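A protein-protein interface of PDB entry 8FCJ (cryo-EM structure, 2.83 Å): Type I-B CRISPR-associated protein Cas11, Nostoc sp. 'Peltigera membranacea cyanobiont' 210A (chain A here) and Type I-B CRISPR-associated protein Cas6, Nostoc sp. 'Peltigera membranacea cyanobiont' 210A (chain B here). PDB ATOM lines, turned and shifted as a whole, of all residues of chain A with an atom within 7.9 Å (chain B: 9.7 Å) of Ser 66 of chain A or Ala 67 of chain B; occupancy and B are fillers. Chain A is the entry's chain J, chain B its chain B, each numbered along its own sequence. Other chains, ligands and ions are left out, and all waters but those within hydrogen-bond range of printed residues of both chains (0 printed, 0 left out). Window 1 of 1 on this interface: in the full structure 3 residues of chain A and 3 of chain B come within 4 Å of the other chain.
The guanidinium group of Arg 19 of chain B is in salt-bridge range of the side-chain carboxylate of Glu 63 of chain A, at 3.0 Å.
The side-chain hydroxyl (OG1) of Thr 66 of chain B is in hydrogen-bond range of the side-chain amide oxygen (OE1) of Gln 68 of chain B (2.7 Å).
O of Lys 62 of chain A sits at hydrogen-bond distance from OG of Ser 66 of chain A (3.2 Å).
The backbone carbonyl oxygen (O) of Leu 59 of chain A sits close to the side-chain carboxylate (OE1) of Glu 63 of chain A, at 2.5 Å.
Among the printed residues, pairs that only touch across the chains: Leu 59 of chain A with Arg 19 of chain B, Ser 66 of chain A with Ala 67 of chain B and Ser 66 of chain A with Gln 68 of chain B.
Printed residues of chain B within 4 Å of Ser 66 of chain A: Ala 67 (3.9 Å) and Gln 68 (3.8 Å).
Ala 67 of chain B touches just one residue of chain A: Ser 66 (3.9 Å).
Glu 63 of chain A touches one residue of chain B.
Of the printed residues of chain A, Arg 19 of chain B touches Leu 59 (3.5 Å) and Glu 63 (3.0 Å).
Of the printed residues of chain A, Gln 68 of chain B touches Ser 66.
Of the printed residues of chain B, Leu 59 of chain A touches Arg 19 (3.5 Å).
The nearest residue of chain B that does not touch Ser 66 of chain A is Thr 66 of chain B (6.8 Å).
The nearest residue of chain A that does not touch Ala 67 of chain B is Glu 63 of chain A (4.4 Å).
Hydrophobic or aromatic side chains of chain A that line the printed part of chain B: Leu 59.
Of the 19 printed residues of chain B, 3 touch a printed residue of chain A.
Printed residues of chain B that touch a printed residue of chain A: Arg 19, Ala 67 and Gln 68.
Hydrophobic or aromatic side chains of chain B that line the printed part of chain A: Ala 67.
Among the printed residues, 4 pairs touch across the chains.
Among the printed residues, Asp or Glu carboxylates within 4 Å of a Lys or Arg side-chain nitrogen of the other chain: Glu 63 of chain A with Arg 19 of chain B (3.0 Å).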
ATOM      1  N   LEU A  59     -25.587 -29.443  -5.568  1.00  0.00           N
ATOM      2  CA  LEU A  59     -26.287 -28.172  -5.396  1.00  0.00           C
ATOM      3  C   LEU A  59     -26.123 -27.643  -3.974  1.00  0.00           C
ATOM      4  O   LEU A  59     -25.538 -26.572  -3.744  1.00  0.00           O
ATOM      5  CB  LEU A  59     -27.771 -28.366  -5.721  1.00  0.00           C
ATOM      6  CG  LEU A  59     -28.322 -28.206  -7.144  1.00  0.00           C
ATOM      7  CD1 LEU A  59     -28.666 -26.762  -7.456  1.00  0.00           C
ATOM      8  CD2 LEU A  59     -27.358 -28.763  -8.171  1.00  0.00           C
ATOM      9  N   PHE A  61     -24.390 -27.256  -0.498  1.00  0.00           N
ATOM     10  CA  PHE A  61     -23.003 -27.022  -0.115  1.00  0.00           C
ATOM     11  C   PHE A  61     -22.196 -26.347  -1.216  1.00  0.00           C
ATOM     12  O   PHE A  61     -21.302 -25.566  -0.895  1.00  0.00           O
ATOM     13  CB  PHE A  61     -22.316 -28.330   0.294  1.00  0.00           C
ATOM     14  CG  PHE A  61     -20.838 -28.203   0.473  1.00  0.00           C
ATOM     15  CD1 PHE A  61     -20.318 -27.690   1.644  1.00  0.00           C
ATOM     16  CD2 PHE A  61     -19.968 -28.599  -0.525  1.00  0.00           C
ATOM     17  CE1 PHE A  61     -18.962 -27.564   1.815  1.00  0.00           C
ATOM     18  CE2 PHE A  61     -18.610 -28.476  -0.357  1.00  0.00           C
ATOM     19  CZ  PHE A  61     -18.108 -27.960   0.816  1.00  0.00           C
ATOM     20  N   LYS A  62     -22.630 -26.417  -2.473  1.00  0.00           N
ATOM     21  CA  LYS A  62     -21.909 -25.656  -3.490  1.00  0.00           C
ATOM     22  C   LYS A  62     -22.427 -24.227  -3.536  1.00  0.00           C
ATOM     23  O   LYS A  62     -21.653 -23.276  -3.371  1.00  0.00           O
ATOM     24  CB  LYS A  62     -22.008 -26.311  -4.869  1.00  0.00           C
ATOM     25  CG  LYS A  62     -21.021 -27.445  -5.081  1.00  0.00           C
ATOM     26  CD  LYS A  62     -19.596 -26.946  -4.967  1.00  0.00           C
ATOM     27  CE  LYS A  62     -18.598 -28.009  -5.389  1.00  0.00           C
ATOM     28  NZ  LYS A  62     -19.094 -28.837  -6.521  1.00  0.00           N
ATOM     29  N   GLU A  63     -23.737 -24.060  -3.742  1.00  0.00           N
ATOM     30  CA  GLU A  63     -24.287 -22.727  -3.522  1.00  0.00           C
ATOM     31  C   GLU A  63     -24.111 -22.264  -2.082  1.00  0.00           C
ATOM     32  O   GLU A  63     -23.892 -21.071  -1.852  1.00  0.00           O
ATOM     33  CB  GLU A  63     -25.745 -22.643  -3.979  1.00  0.00           C
ATOM     34  CG  GLU A  63     -26.006 -22.854  -5.486  1.00  0.00           C
ATOM     35  CD  GLU A  63     -25.739 -24.237  -6.034  1.00  0.00           C
ATOM     36  OE1 GLU A  63     -24.842 -24.940  -5.538  1.00  0.00           O
ATOM     37  OE2 GLU A  63     -26.429 -24.618  -6.998  1.00  0.00           O
ATOM     38  N   TYR A  64     -24.144 -23.175  -1.105  1.00  0.00           N
ATOM     39  CA  TYR A  64     -23.900 -22.750   0.272  1.00  0.00           C
ATOM     40  C   TYR A  64     -22.519 -22.128   0.429  1.00  0.00           C
ATOM     41  O   TYR A  64     -22.386 -21.024   0.968  1.00  0.00           O
ATOM     42  CB  TYR A  64     -24.053 -23.907   1.253  1.00  0.00           C
ATOM     43  CG  TYR A  64     -23.777 -23.467   2.674  1.00  0.00           C
ATOM     44  CD1 TYR A  64     -24.705 -22.720   3.385  1.00  0.00           C
ATOM     45  CD2 TYR A  64     -22.567 -23.761   3.287  1.00  0.00           C
ATOM     46  CE1 TYR A  64     -24.446 -22.303   4.675  1.00  0.00           C
ATOM     47  CE2 TYR A  64     -22.299 -23.347   4.574  1.00  0.00           C
ATOM     48  CZ  TYR A  64     -23.243 -22.619   5.263  1.00  0.00           C
ATOM     49  OH  TYR A  64     -22.983 -22.202   6.546  1.00  0.00           O
ATOM     50  N   LEU A  65     -21.472 -22.813  -0.034  1.00  0.00           N
ATOM     51  CA  LEU A  65     -20.132 -22.304   0.199  1.00  0.00           C
ATOM     52  C   LEU A  65     -19.815 -21.116  -0.697  1.00  0.00           C
ATOM     53  O   LEU A  65     -19.071 -20.221  -0.284  1.00  0.00           O
ATOM     54  CB  LEU A  65     -19.111 -23.424   0.010  1.00  0.00           C
ATOM     55  CG  LEU A  65     -17.666 -23.029   0.276  1.00  0.00           C
ATOM     56  CD1 LEU A  65     -17.237 -23.595   1.607  1.00  0.00           C
ATOM     57  CD2 LEU A  65     -16.791 -23.559  -0.811  1.00  0.00           C
ATOM     58  N   SER A  66     -20.377 -21.071  -1.909  1.00  0.00           N
ATOM     59  CA  SER A  66     -20.223 -19.876  -2.732  1.00  0.00           C
ATOM     60  C   SER A  66     -20.866 -18.666  -2.065  1.00  0.00           C
ATOM     61  O   SER A  66     -20.280 -17.577  -2.040  1.00  0.00           O
ATOM     62  CB  SER A  66     -20.822 -20.111  -4.117  1.00  0.00           C
ATOM     63  OG  SER A  66     -20.015 -20.993  -4.875  1.00  0.00           O
ATOM     64  N   ASP A  67     -22.064 -18.843  -1.502  1.00  0.00           N
ATOM     65  CA  ASP A  67     -22.728 -17.751  -0.802  1.00  0.00           C
ATOM     66  C   ASP A  67     -21.923 -17.349   0.429  1.00  0.00           C
ATOM     67  O   ASP A  67     -21.791 -16.159   0.737  1.00  0.00           O
ATOM     68  CB  ASP A  67     -24.152 -18.194  -0.436  1.00  0.00           C
ATOM     69  CG  ASP A  67     -24.941 -17.152   0.352  1.00  0.00           C
ATOM     70  OD1 ASP A  67     -24.408 -16.086   0.710  1.00  0.00           O
ATOM     71  OD2 ASP A  67     -26.131 -17.414   0.623  1.00  0.00           O
ATOM     72  N   PHE A  68     -21.360 -18.333   1.134  1.00  0.00           N
ATOM     73  CA  PHE A  68     -20.527 -18.053   2.300  1.00  0.00           C
ATOM     74  C   PHE A  68     -19.317 -17.208   1.922  1.00  0.00           C
ATOM     75  O   PHE A  68     -19.007 -16.209   2.581  1.00  0.00           O
ATOM     76  CB  PHE A  68     -20.090 -19.373   2.939  1.00  0.00           C
ATOM     77  CG  PHE A  68     -19.239 -19.214   4.164  1.00  0.00           C
ATOM     78  CD1 PHE A  68     -19.817 -19.070   5.411  1.00  0.00           C
ATOM     79  CD2 PHE A  68     -17.858 -19.230   4.070  1.00  0.00           C
ATOM     80  CE1 PHE A  68     -19.036 -18.934   6.540  1.00  0.00           C
ATOM     81  CE2 PHE A  68     -17.074 -19.091   5.196  1.00  0.00           C
ATOM     82  CZ  PHE A  68     -17.664 -18.943   6.430  1.00  0.00           C
ATOM     83  N   LEU A  69     -18.625 -17.592   0.848  1.00  0.00           N
ATOM     84  CA  LEU A  69     -17.470 -16.822   0.401  1.00  0.00           C
ATOM     85  C   LEU A  69     -17.880 -15.425  -0.049  1.00  0.00           C
ATOM     86  O   LEU A  69     -17.142 -14.457   0.169  1.00  0.00           O
ATOM     87  CB  LEU A  69     -16.747 -17.560  -0.724  1.00  0.00           C
ATOM     88  CG  LEU A  69     -16.073 -18.876  -0.334  1.00  0.00           C
ATOM     89  CD1 LEU A  69     -15.217 -19.399  -1.474  1.00  0.00           C
ATOM     90  CD2 LEU A  69     -15.245 -18.701   0.925  1.00  0.00           C
ATOM     91  N   VAL A  70     -19.048 -15.300  -0.681  1.00  0.00           N
ATOM     92  CA  VAL A  70     -19.515 -13.986  -1.114  1.00  0.00           C
ATOM     93  C   VAL A  70     -19.764 -13.084   0.092  1.00  0.00           C
ATOM     94  O   VAL A  70     -19.331 -11.927   0.118  1.00  0.00           O
ATOM     95  CB  VAL A  70     -20.771 -14.125  -1.993  1.00  0.00           C
ATOM     96  CG1 VAL A  70     -21.644 -12.886  -1.885  1.00  0.00           C
ATOM     97  CG2 VAL A  70     -20.372 -14.376  -3.438  1.00  0.00           C
ATOM     98  N   ARG A  71     -20.450 -13.603   1.114  1.00  0.00           N
ATOM     99  CA  ARG A  71     -20.630 -12.821   2.334  1.00  0.00           C
ATOM    100  C   ARG A  71     -19.337 -12.646   3.114  1.00  0.00           C
ATOM    101  O   ARG A  71     -19.310 -11.843   4.053  1.00  0.00           O
ATOM    102  CB  ARG A  71     -21.678 -13.439   3.259  1.00  0.00           C
ATOM    103  CG  ARG A  71     -22.918 -13.980   2.582  1.00  0.00           C
ATOM    104  CD  ARG A  71     -23.674 -14.971   3.483  1.00  0.00           C
ATOM    105  NE  ARG A  71     -23.711 -14.646   4.909  1.00  0.00           N
ATOM    106  CZ  ARG A  71     -24.077 -13.483   5.436  1.00  0.00           C
ATOM    107  NH1 ARG A  71     -24.526 -12.487   4.688  1.00  0.00           N
ATOM    108  NH2 ARG A  71     -24.012 -13.321   6.754  1.00  0.00           N
ATOM    109  N   GLY A  72     -18.278 -13.376   2.763  1.00  0.00           N
ATOM    110  CA  GLY A  72     -16.991 -13.149   3.395  1.00  0.00           C
ATOM    111  C   GLY A  72     -16.497 -11.724   3.270  1.00  0.00           C
ATOM    112  O   GLY A  72     -15.733 -11.264   4.125  1.00  0.00           O
ATOM    113  N   PHE A  78      -8.756 -13.822  -2.017  1.00  0.00           N
ATOM    114  CA  PHE A  78      -9.774 -14.166  -3.000  1.00  0.00           C
ATOM    115  C   PHE A  78      -9.582 -13.359  -4.282  1.00  0.00           C
ATOM    116  O   PHE A  78      -9.677 -13.906  -5.386  1.00  0.00           O
ATOM    117  CB  PHE A  78     -11.163 -13.930  -2.405  1.00  0.00           C
ATOM    118  CG  PHE A  78     -12.247 -14.778  -3.013  1.00  0.00           C
ATOM    119  CD1 PHE A  78     -12.042 -15.451  -4.205  1.00  0.00           C
ATOM    120  CD2 PHE A  78     -13.463 -14.928  -2.367  1.00  0.00           C
ATOM    121  CE1 PHE A  78     -13.037 -16.233  -4.754  1.00  0.00           C
ATOM    122  CE2 PHE A  78     -14.462 -15.710  -2.912  1.00  0.00           C
ATOM    123  CZ  PHE A  78     -14.248 -16.364  -4.105  1.00  0.00           C
ATOM    124  N   ALA A  86     -12.167 -20.773  -8.280  1.00  0.00           N
ATOM    125  CA  ALA A  86     -13.431 -21.141  -8.907  1.00  0.00           C
ATOM    126  C   ALA A  86     -13.298 -22.454  -9.666  1.00  0.00           C
ATOM    127  O   ALA A  86     -14.196 -23.303  -9.617  1.00  0.00           O
ATOM    128  CB  ALA A  86     -13.902 -20.024  -9.837  1.00  0.00           C
ATOM    129  N   ILE A  89     -13.221 -25.258  -7.153  1.00  0.00           N
ATOM    130  CA  ILE A  89     -14.542 -25.531  -6.598  1.00  0.00           C
ATOM    131  C   ILE A  89     -15.393 -26.289  -7.610  1.00  0.00           C
ATOM    132  O   ILE A  89     -16.104 -27.239  -7.262  1.00  0.00           O
ATOM    133  CB  ILE A  89     -15.218 -24.221  -6.162  1.00  0.00           C
ATOM    134  CG1 ILE A  89     -14.442 -23.609  -4.997  1.00  0.00           C
ATOM    135  CG2 ILE A  89     -16.676 -24.465  -5.796  1.00  0.00           C
ATOM    136  CD1 ILE A  89     -14.981 -23.950  -3.661  1.00  0.00           C
ATOM    137  N   LYS A  90     -15.328 -25.882  -8.879  1.00  0.00           N
ATOM    138  CA  LYS A  90     -16.101 -26.563  -9.912  1.00  0.00           C
ATOM    139  C   LYS A  90     -15.668 -28.016 -10.057  1.00  0.00           C
ATOM    140  O   LYS A  90     -16.509 -28.907 -10.227  1.00  0.00           O
ATOM    141  CB  LYS A  90     -15.969 -25.822 -11.242  1.00  0.00           C
ATOM    142  CG  LYS A  90     -17.216 -25.884 -12.110  1.00  0.00           C
ATOM    143  CD  LYS A  90     -16.905 -25.524 -13.552  1.00  0.00           C
ATOM    144  CE  LYS A  90     -15.960 -26.534 -14.182  1.00  0.00           C
ATOM    145  NZ  LYS A  90     -16.684 -27.729 -14.694  1.00  0.00           N
ATOM    146  N   THR B  15     -34.039 -12.006 -11.315  1.00  0.00           N
ATOM    147  CA  THR B  15     -32.814 -12.788 -11.432  1.00  0.00           C
ATOM    148  C   THR B  15     -33.108 -14.248 -11.121  1.00  0.00           C
ATOM    149  O   THR B  15     -33.540 -14.574 -10.012  1.00  0.00           O
ATOM    150  CB  THR B  15     -31.735 -12.257 -10.488  1.00  0.00           C
ATOM    151  OG1 THR B  15     -31.921 -12.822  -9.185  1.00  0.00           O
ATOM    152  CG2 THR B  15     -31.814 -10.745 -10.389  1.00  0.00           C
ATOM    153  N   PHE B  16     -32.853 -15.120 -12.091  1.00  0.00           N
ATOM    154  CA  PHE B  16     -33.007 -16.559 -11.933  1.00  0.00           C
ATOM    155  C   PHE B  16     -31.629 -17.198 -11.874  1.00  0.00           C
ATOM    156  O   PHE B  16     -30.794 -16.951 -12.748  1.00  0.00           O
ATOM    157  CB  PHE B  16     -33.796 -17.175 -13.093  1.00  0.00           C
ATOM    158  CG  PHE B  16     -35.164 -16.591 -13.291  1.00  0.00           C
ATOM    159  CD1 PHE B  16     -35.331 -15.343 -13.862  1.00  0.00           C
ATOM    160  CD2 PHE B  16     -36.288 -17.312 -12.934  1.00  0.00           C
ATOM    161  CE1 PHE B  16     -36.591 -14.818 -14.054  1.00  0.00           C
ATOM    162  CE2 PHE B  16     -37.548 -16.792 -13.124  1.00  0.00           C
ATOM    163  CZ  PHE B  16     -37.700 -15.544 -13.683  1.00  0.00           C
ATOM    164  N   LYS B  17     -31.393 -18.021 -10.855  1.00  0.00           N
ATOM    165  CA  LYS B  17     -30.152 -18.782 -10.803  1.00  0.00           C
ATOM    166  C   LYS B  17     -30.080 -19.724 -11.998  1.00  0.00           C
ATOM    167  O   LYS B  17     -31.030 -20.459 -12.283  1.00  0.00           O
ATOM    168  CB  LYS B  17     -30.063 -19.571  -9.499  1.00  0.00           C
ATOM    169  CG  LYS B  17     -29.795 -18.722  -8.269  1.00  0.00           C
ATOM    170  CD  LYS B  17     -28.385 -18.941  -7.748  1.00  0.00           C
ATOM    171  CE  LYS B  17     -28.295 -18.637  -6.262  1.00  0.00           C
ATOM    172  NZ  LYS B  17     -28.832 -17.288  -5.938  1.00  0.00           N
ATOM    173  N   LEU B  18     -28.949 -19.703 -12.696  1.00  0.00           N
ATOM    174  CA  LEU B  18     -28.789 -20.423 -13.952  1.00  0.00           C
ATOM    175  C   LEU B  18     -27.708 -21.482 -13.806  1.00  0.00           C
ATOM    176  O   LEU B  18     -26.631 -21.205 -13.270  1.00  0.00           O
ATOM    177  CB  LEU B  18     -28.438 -19.460 -15.091  1.00  0.00           C
ATOM    178  CG  LEU B  18     -28.546 -20.017 -16.509  1.00  0.00           C
ATOM    179  CD1 LEU B  18     -29.794 -20.868 -16.660  1.00  0.00           C
ATOM    180  CD2 LEU B  18     -28.554 -18.881 -17.515  1.00  0.00           C
ATOM    181  N   ARG B  19     -28.004 -22.689 -14.281  1.00  0.00           N
ATOM    182  CA  ARG B  19     -27.060 -23.794 -14.249  1.00  0.00           C
ATOM    183  C   ARG B  19     -27.292 -24.687 -15.459  1.00  0.00           C
ATOM    184  O   ARG B  19     -28.410 -24.796 -15.964  1.00  0.00           O
ATOM    185  CB  ARG B  19     -27.189 -24.608 -12.958  1.00  0.00           C
ATOM    186  CG  ARG B  19     -28.533 -25.300 -12.792  1.00  0.00           C
ATOM    187  CD  ARG B  19     -28.831 -25.851 -11.383  1.00  0.00           C
ATOM    188  NE  ARG B  19     -28.986 -24.855 -10.322  1.00  0.00           N
ATOM    189  CZ  ARG B  19     -28.011 -24.146  -9.763  1.00  0.00           C
ATOM    190  NH1 ARG B  19     -26.735 -24.395 -10.012  1.00  0.00           N
ATOM    191  NH2 ARG B  19     -28.324 -23.194  -8.890  1.00  0.00           N
ATOM    192  N   GLY B  20     -26.225 -25.322 -15.919  1.00  0.00           N
ATOM    193  CA  GLY B  20     -26.318 -26.210 -17.058  1.00  0.00           C
ATOM    194  C   GLY B  20     -24.963 -26.395 -17.715  1.00  0.00           C
ATOM    195  O   GLY B  20     -23.915 -26.106 -17.134  1.00  0.00           O
ATOM    196  N   ILE B  53     -25.280 -12.928 -19.453  1.00  0.00           N
ATOM    197  CA  ILE B  53     -24.994 -13.909 -18.416  1.00  0.00           C
ATOM    198  C   ILE B  53     -23.589 -13.688 -17.877  1.00  0.00           C
ATOM    199  O   ILE B  53     -22.624 -13.537 -18.636  1.00  0.00           O
ATOM    200  CB  ILE B  53     -25.167 -15.333 -18.965  1.00  0.00           C
ATOM    201  CG1 ILE B  53     -26.520 -15.463 -19.667  1.00  0.00           C
ATOM    202  CG2 ILE B  53     -25.048 -16.348 -17.845  1.00  0.00           C
ATOM    203  CD1 ILE B  53     -26.860 -16.873 -20.087  1.00  0.00           C
ATOM    204  N   ALA B  54     -23.471 -13.665 -16.552  1.00  0.00           N
ATOM    205  CA  ALA B  54     -22.208 -13.386 -15.880  1.00  0.00           C
ATOM    206  C   ALA B  54     -21.555 -14.704 -15.482  1.00  0.00           C
ATOM    207  O   ALA B  54     -22.011 -15.376 -14.552  1.00  0.00           O
ATOM    208  CB  ALA B  54     -22.426 -12.490 -14.663  1.00  0.00           C
ATOM    209  N   GLY B  55     -20.484 -15.062 -16.180  1.00  0.00           N
ATOM    210  CA  GLY B  55     -19.714 -16.245 -15.850  1.00  0.00           C
ATOM    211  C   GLY B  55     -18.353 -16.157 -16.496  1.00  0.00           C
ATOM    212  O   GLY B  55     -18.166 -15.456 -17.494  1.00  0.00           O
ATOM    213  N   ILE B  56     -17.398 -16.881 -15.919  1.00  0.00           N
ATOM    214  CA  ILE B  56     -16.016 -16.807 -16.385  1.00  0.00           C
ATOM    215  C   ILE B  56     -15.912 -17.348 -17.809  1.00  0.00           C
ATOM    216  O   ILE B  56     -16.724 -18.192 -18.215  1.00  0.00           O
ATOM    217  CB  ILE B  56     -15.056 -17.489 -15.384  1.00  0.00           C
ATOM    218  CG1 ILE B  56     -15.396 -18.959 -15.040  1.00  0.00           C
ATOM    219  CG2 ILE B  56     -14.964 -16.668 -14.103  1.00  0.00           C
ATOM    220  CD1 ILE B  56     -15.498 -19.979 -16.156  1.00  0.00           C
ATOM    221  N   GLU B  64     -18.780 -20.560 -19.468  1.00  0.00           N
ATOM    222  CA  GLU B  64     -19.069 -21.571 -18.460  1.00  0.00           C
ATOM    223  C   GLU B  64     -19.904 -20.976 -17.335  1.00  0.00           C
ATOM    224  O   GLU B  64     -19.591 -19.904 -16.809  1.00  0.00           O
ATOM    225  CB  GLU B  64     -17.776 -22.162 -17.900  1.00  0.00           C
ATOM    226  CG  GLU B  64     -17.970 -23.121 -16.729  1.00  0.00           C
ATOM    227  CD  GLU B  64     -18.927 -24.258 -17.043  1.00  0.00           C
ATOM    228  OE1 GLU B  64     -20.157 -24.065 -16.914  1.00  0.00           O
ATOM    229  OE2 GLU B  64     -18.450 -25.349 -17.418  1.00  0.00           O
ATOM    230  N   LEU B  65     -20.968 -21.685 -16.967  1.00  0.00           N
ATOM    231  CA  LEU B  65     -21.904 -21.218 -15.954  1.00  0.00           C
ATOM    232  C   LEU B  65     -21.395 -21.575 -14.565  1.00  0.00           C
ATOM    233  O   LEU B  65     -21.071 -22.736 -14.292  1.00  0.00           O
ATOM    234  CB  LEU B  65     -23.287 -21.829 -16.181  1.00  0.00           C
ATOM    235  CG  LEU B  65     -24.008 -21.391 -17.456  1.00  0.00           C
ATOM    236  CD1 LEU B  65     -25.325 -22.132 -17.607  1.00  0.00           C
ATOM    237  CD2 LEU B  65     -24.230 -19.890 -17.446  1.00  0.00           C
ATOM    238  N   THR B  66     -21.329 -20.578 -13.690  1.00  0.00           N
ATOM    239  CA  THR B  66     -20.921 -20.770 -12.309  1.00  0.00           C
ATOM    240  C   THR B  66     -22.145 -20.730 -11.398  1.00  0.00           C
ATOM    241  O   THR B  66     -23.274 -20.491 -11.836  1.00  0.00           O
ATOM    242  CB  THR B  66     -19.901 -19.707 -11.892  1.00  0.00           C
ATOM    243  OG1 THR B  66     -20.574 -18.632 -11.226  1.00  0.00           O
ATOM    244  CG2 THR B  66     -19.171 -19.163 -13.110  1.00  0.00           C
ATOM    245  N   ALA B  67     -21.915 -20.972 -10.106  1.00  0.00           N
ATOM    246  CA  ALA B  67     -22.991 -20.831  -9.133  1.00  0.00           C
ATOM    247  C   ALA B  67     -23.450 -19.383  -9.025  1.00  0.00           C
ATOM    248  O   ALA B  67     -24.598 -19.121  -8.649  1.00  0.00           O
ATOM    249  CB  ALA B  67     -22.544 -21.351  -7.768  1.00  0.00           C
ATOM    250  N   GLN B  68     -22.571 -18.436  -9.348  1.00  0.00           N
ATOM    251  CA  GLN B  68     -22.921 -17.026  -9.370  1.00  0.00           C
ATOM    252  C   GLN B  68     -23.518 -16.590 -10.701  1.00  0.00           C
ATOM    253  O   GLN B  68     -23.984 -15.451 -10.811  1.00  0.00           O
ATOM    254  CB  GLN B  68     -21.696 -16.149  -9.059  1.00  0.00           C
ATOM    255  CG  GLN B  68     -20.882 -16.484  -7.790  1.00  0.00           C
ATOM    256  CD  GLN B  68     -20.162 -17.829  -7.812  1.00  0.00           C
ATOM    257  OE1 GLN B  68     -20.543 -18.754  -8.526  1.00  0.00           O
ATOM    258  NE2 GLN B  68     -19.105 -17.934  -7.016  1.00  0.00           N
ATOM    259  N   SER B  69     -23.511 -17.462 -11.707  1.00  0.00           N
ATOM    260  CA  SER B  69     -24.133 -17.140 -12.982  1.00  0.00           C
ATOM    261  C   SER B  69     -25.647 -17.212 -12.852  1.00  0.00           C
ATOM    262  O   SER B  69     -26.191 -18.202 -12.351  1.00  0.00           O
ATOM    263  CB  SER B  69     -23.648 -18.099 -14.067  1.00  0.00           C
ATOM    264  OG  SER B  69     -22.233 -18.137 -14.116  1.00  0.00           O
ATOM    265  N   ARG B  70     -26.331 -16.163 -13.300  1.00  0.00           N
ATOM    266  CA  ARG B  70     -27.775 -16.100 -13.156  1.00  0.00           C
ATOM    267  C   ARG B  70     -28.384 -15.366 -14.340  1.00  0.00           C
ATOM    268  O   ARG B  70     -27.803 -14.408 -14.855  1.00  0.00           O
ATOM    269  CB  ARG B  70     -28.171 -15.410 -11.844  1.00  0.00           C
ATOM    270  CG  ARG B  70     -27.677 -13.982 -11.710  1.00  0.00           C
ATOM    271  CD  ARG B  70     -27.831 -13.478 -10.286  1.00  0.00           C
ATOM    272  NE  ARG B  70     -26.960 -14.189  -9.357  1.00  0.00           N
ATOM    273  CZ  ARG B  70     -27.362 -15.153  -8.540  1.00  0.00           C
ATOM    274  NH1 ARG B  70     -28.622 -15.549  -8.508  1.00  0.00           N
ATOM    275  NH2 ARG B  70     -26.476 -15.733  -7.735  1.00  0.00           N
ATOM    276  N   LEU B  71     -29.555 -15.831 -14.767  1.00  0.00           N
ATOM    277  CA  LEU B  71     -30.318 -15.158 -15.808  1.00  0.00           C
ATOM    278  C   LEU B  71     -31.093 -14.006 -15.183  1.00  0.00           C
ATOM    279  O   LEU B  71     -31.933 -14.221 -14.302  1.00  0.00           O
ATOM    280  CB  LEU B  71     -31.260 -16.141 -16.497  1.00  0.00           C
ATOM    281  CG  LEU B  71     -32.490 -15.565 -17.198  1.00  0.00           C
ATOM    282  CD1 LEU B  71     -32.085 -14.777 -18.430  1.00  0.00           C
ATOM    283  CD2 LEU B  71     -33.457 -16.674 -17.565  1.00  0.00           C
ATOM    284  N   ASP B 102     -34.779 -21.575 -10.908  1.00  0.00           N
ATOM    285  CA  ASP B 102     -35.461 -21.670  -9.630  1.00  0.00           C
ATOM    286  C   ASP B 102     -36.290 -20.410  -9.385  1.00  0.00           C
ATOM    287  O   ASP B 102     -36.475 -19.578 -10.278  1.00  0.00           O
ATOM    288  CB  ASP B 102     -34.453 -21.932  -8.507  1.00  0.00           C
ATOM    289  CG  ASP B 102     -33.347 -20.893  -8.444  1.00  0.00           C
ATOM    290  OD1 ASP B 102     -33.571 -19.729  -8.836  1.00  0.00           O
ATOM    291  OD2 ASP B 102     -32.239 -21.252  -7.998  1.00  0.00           O
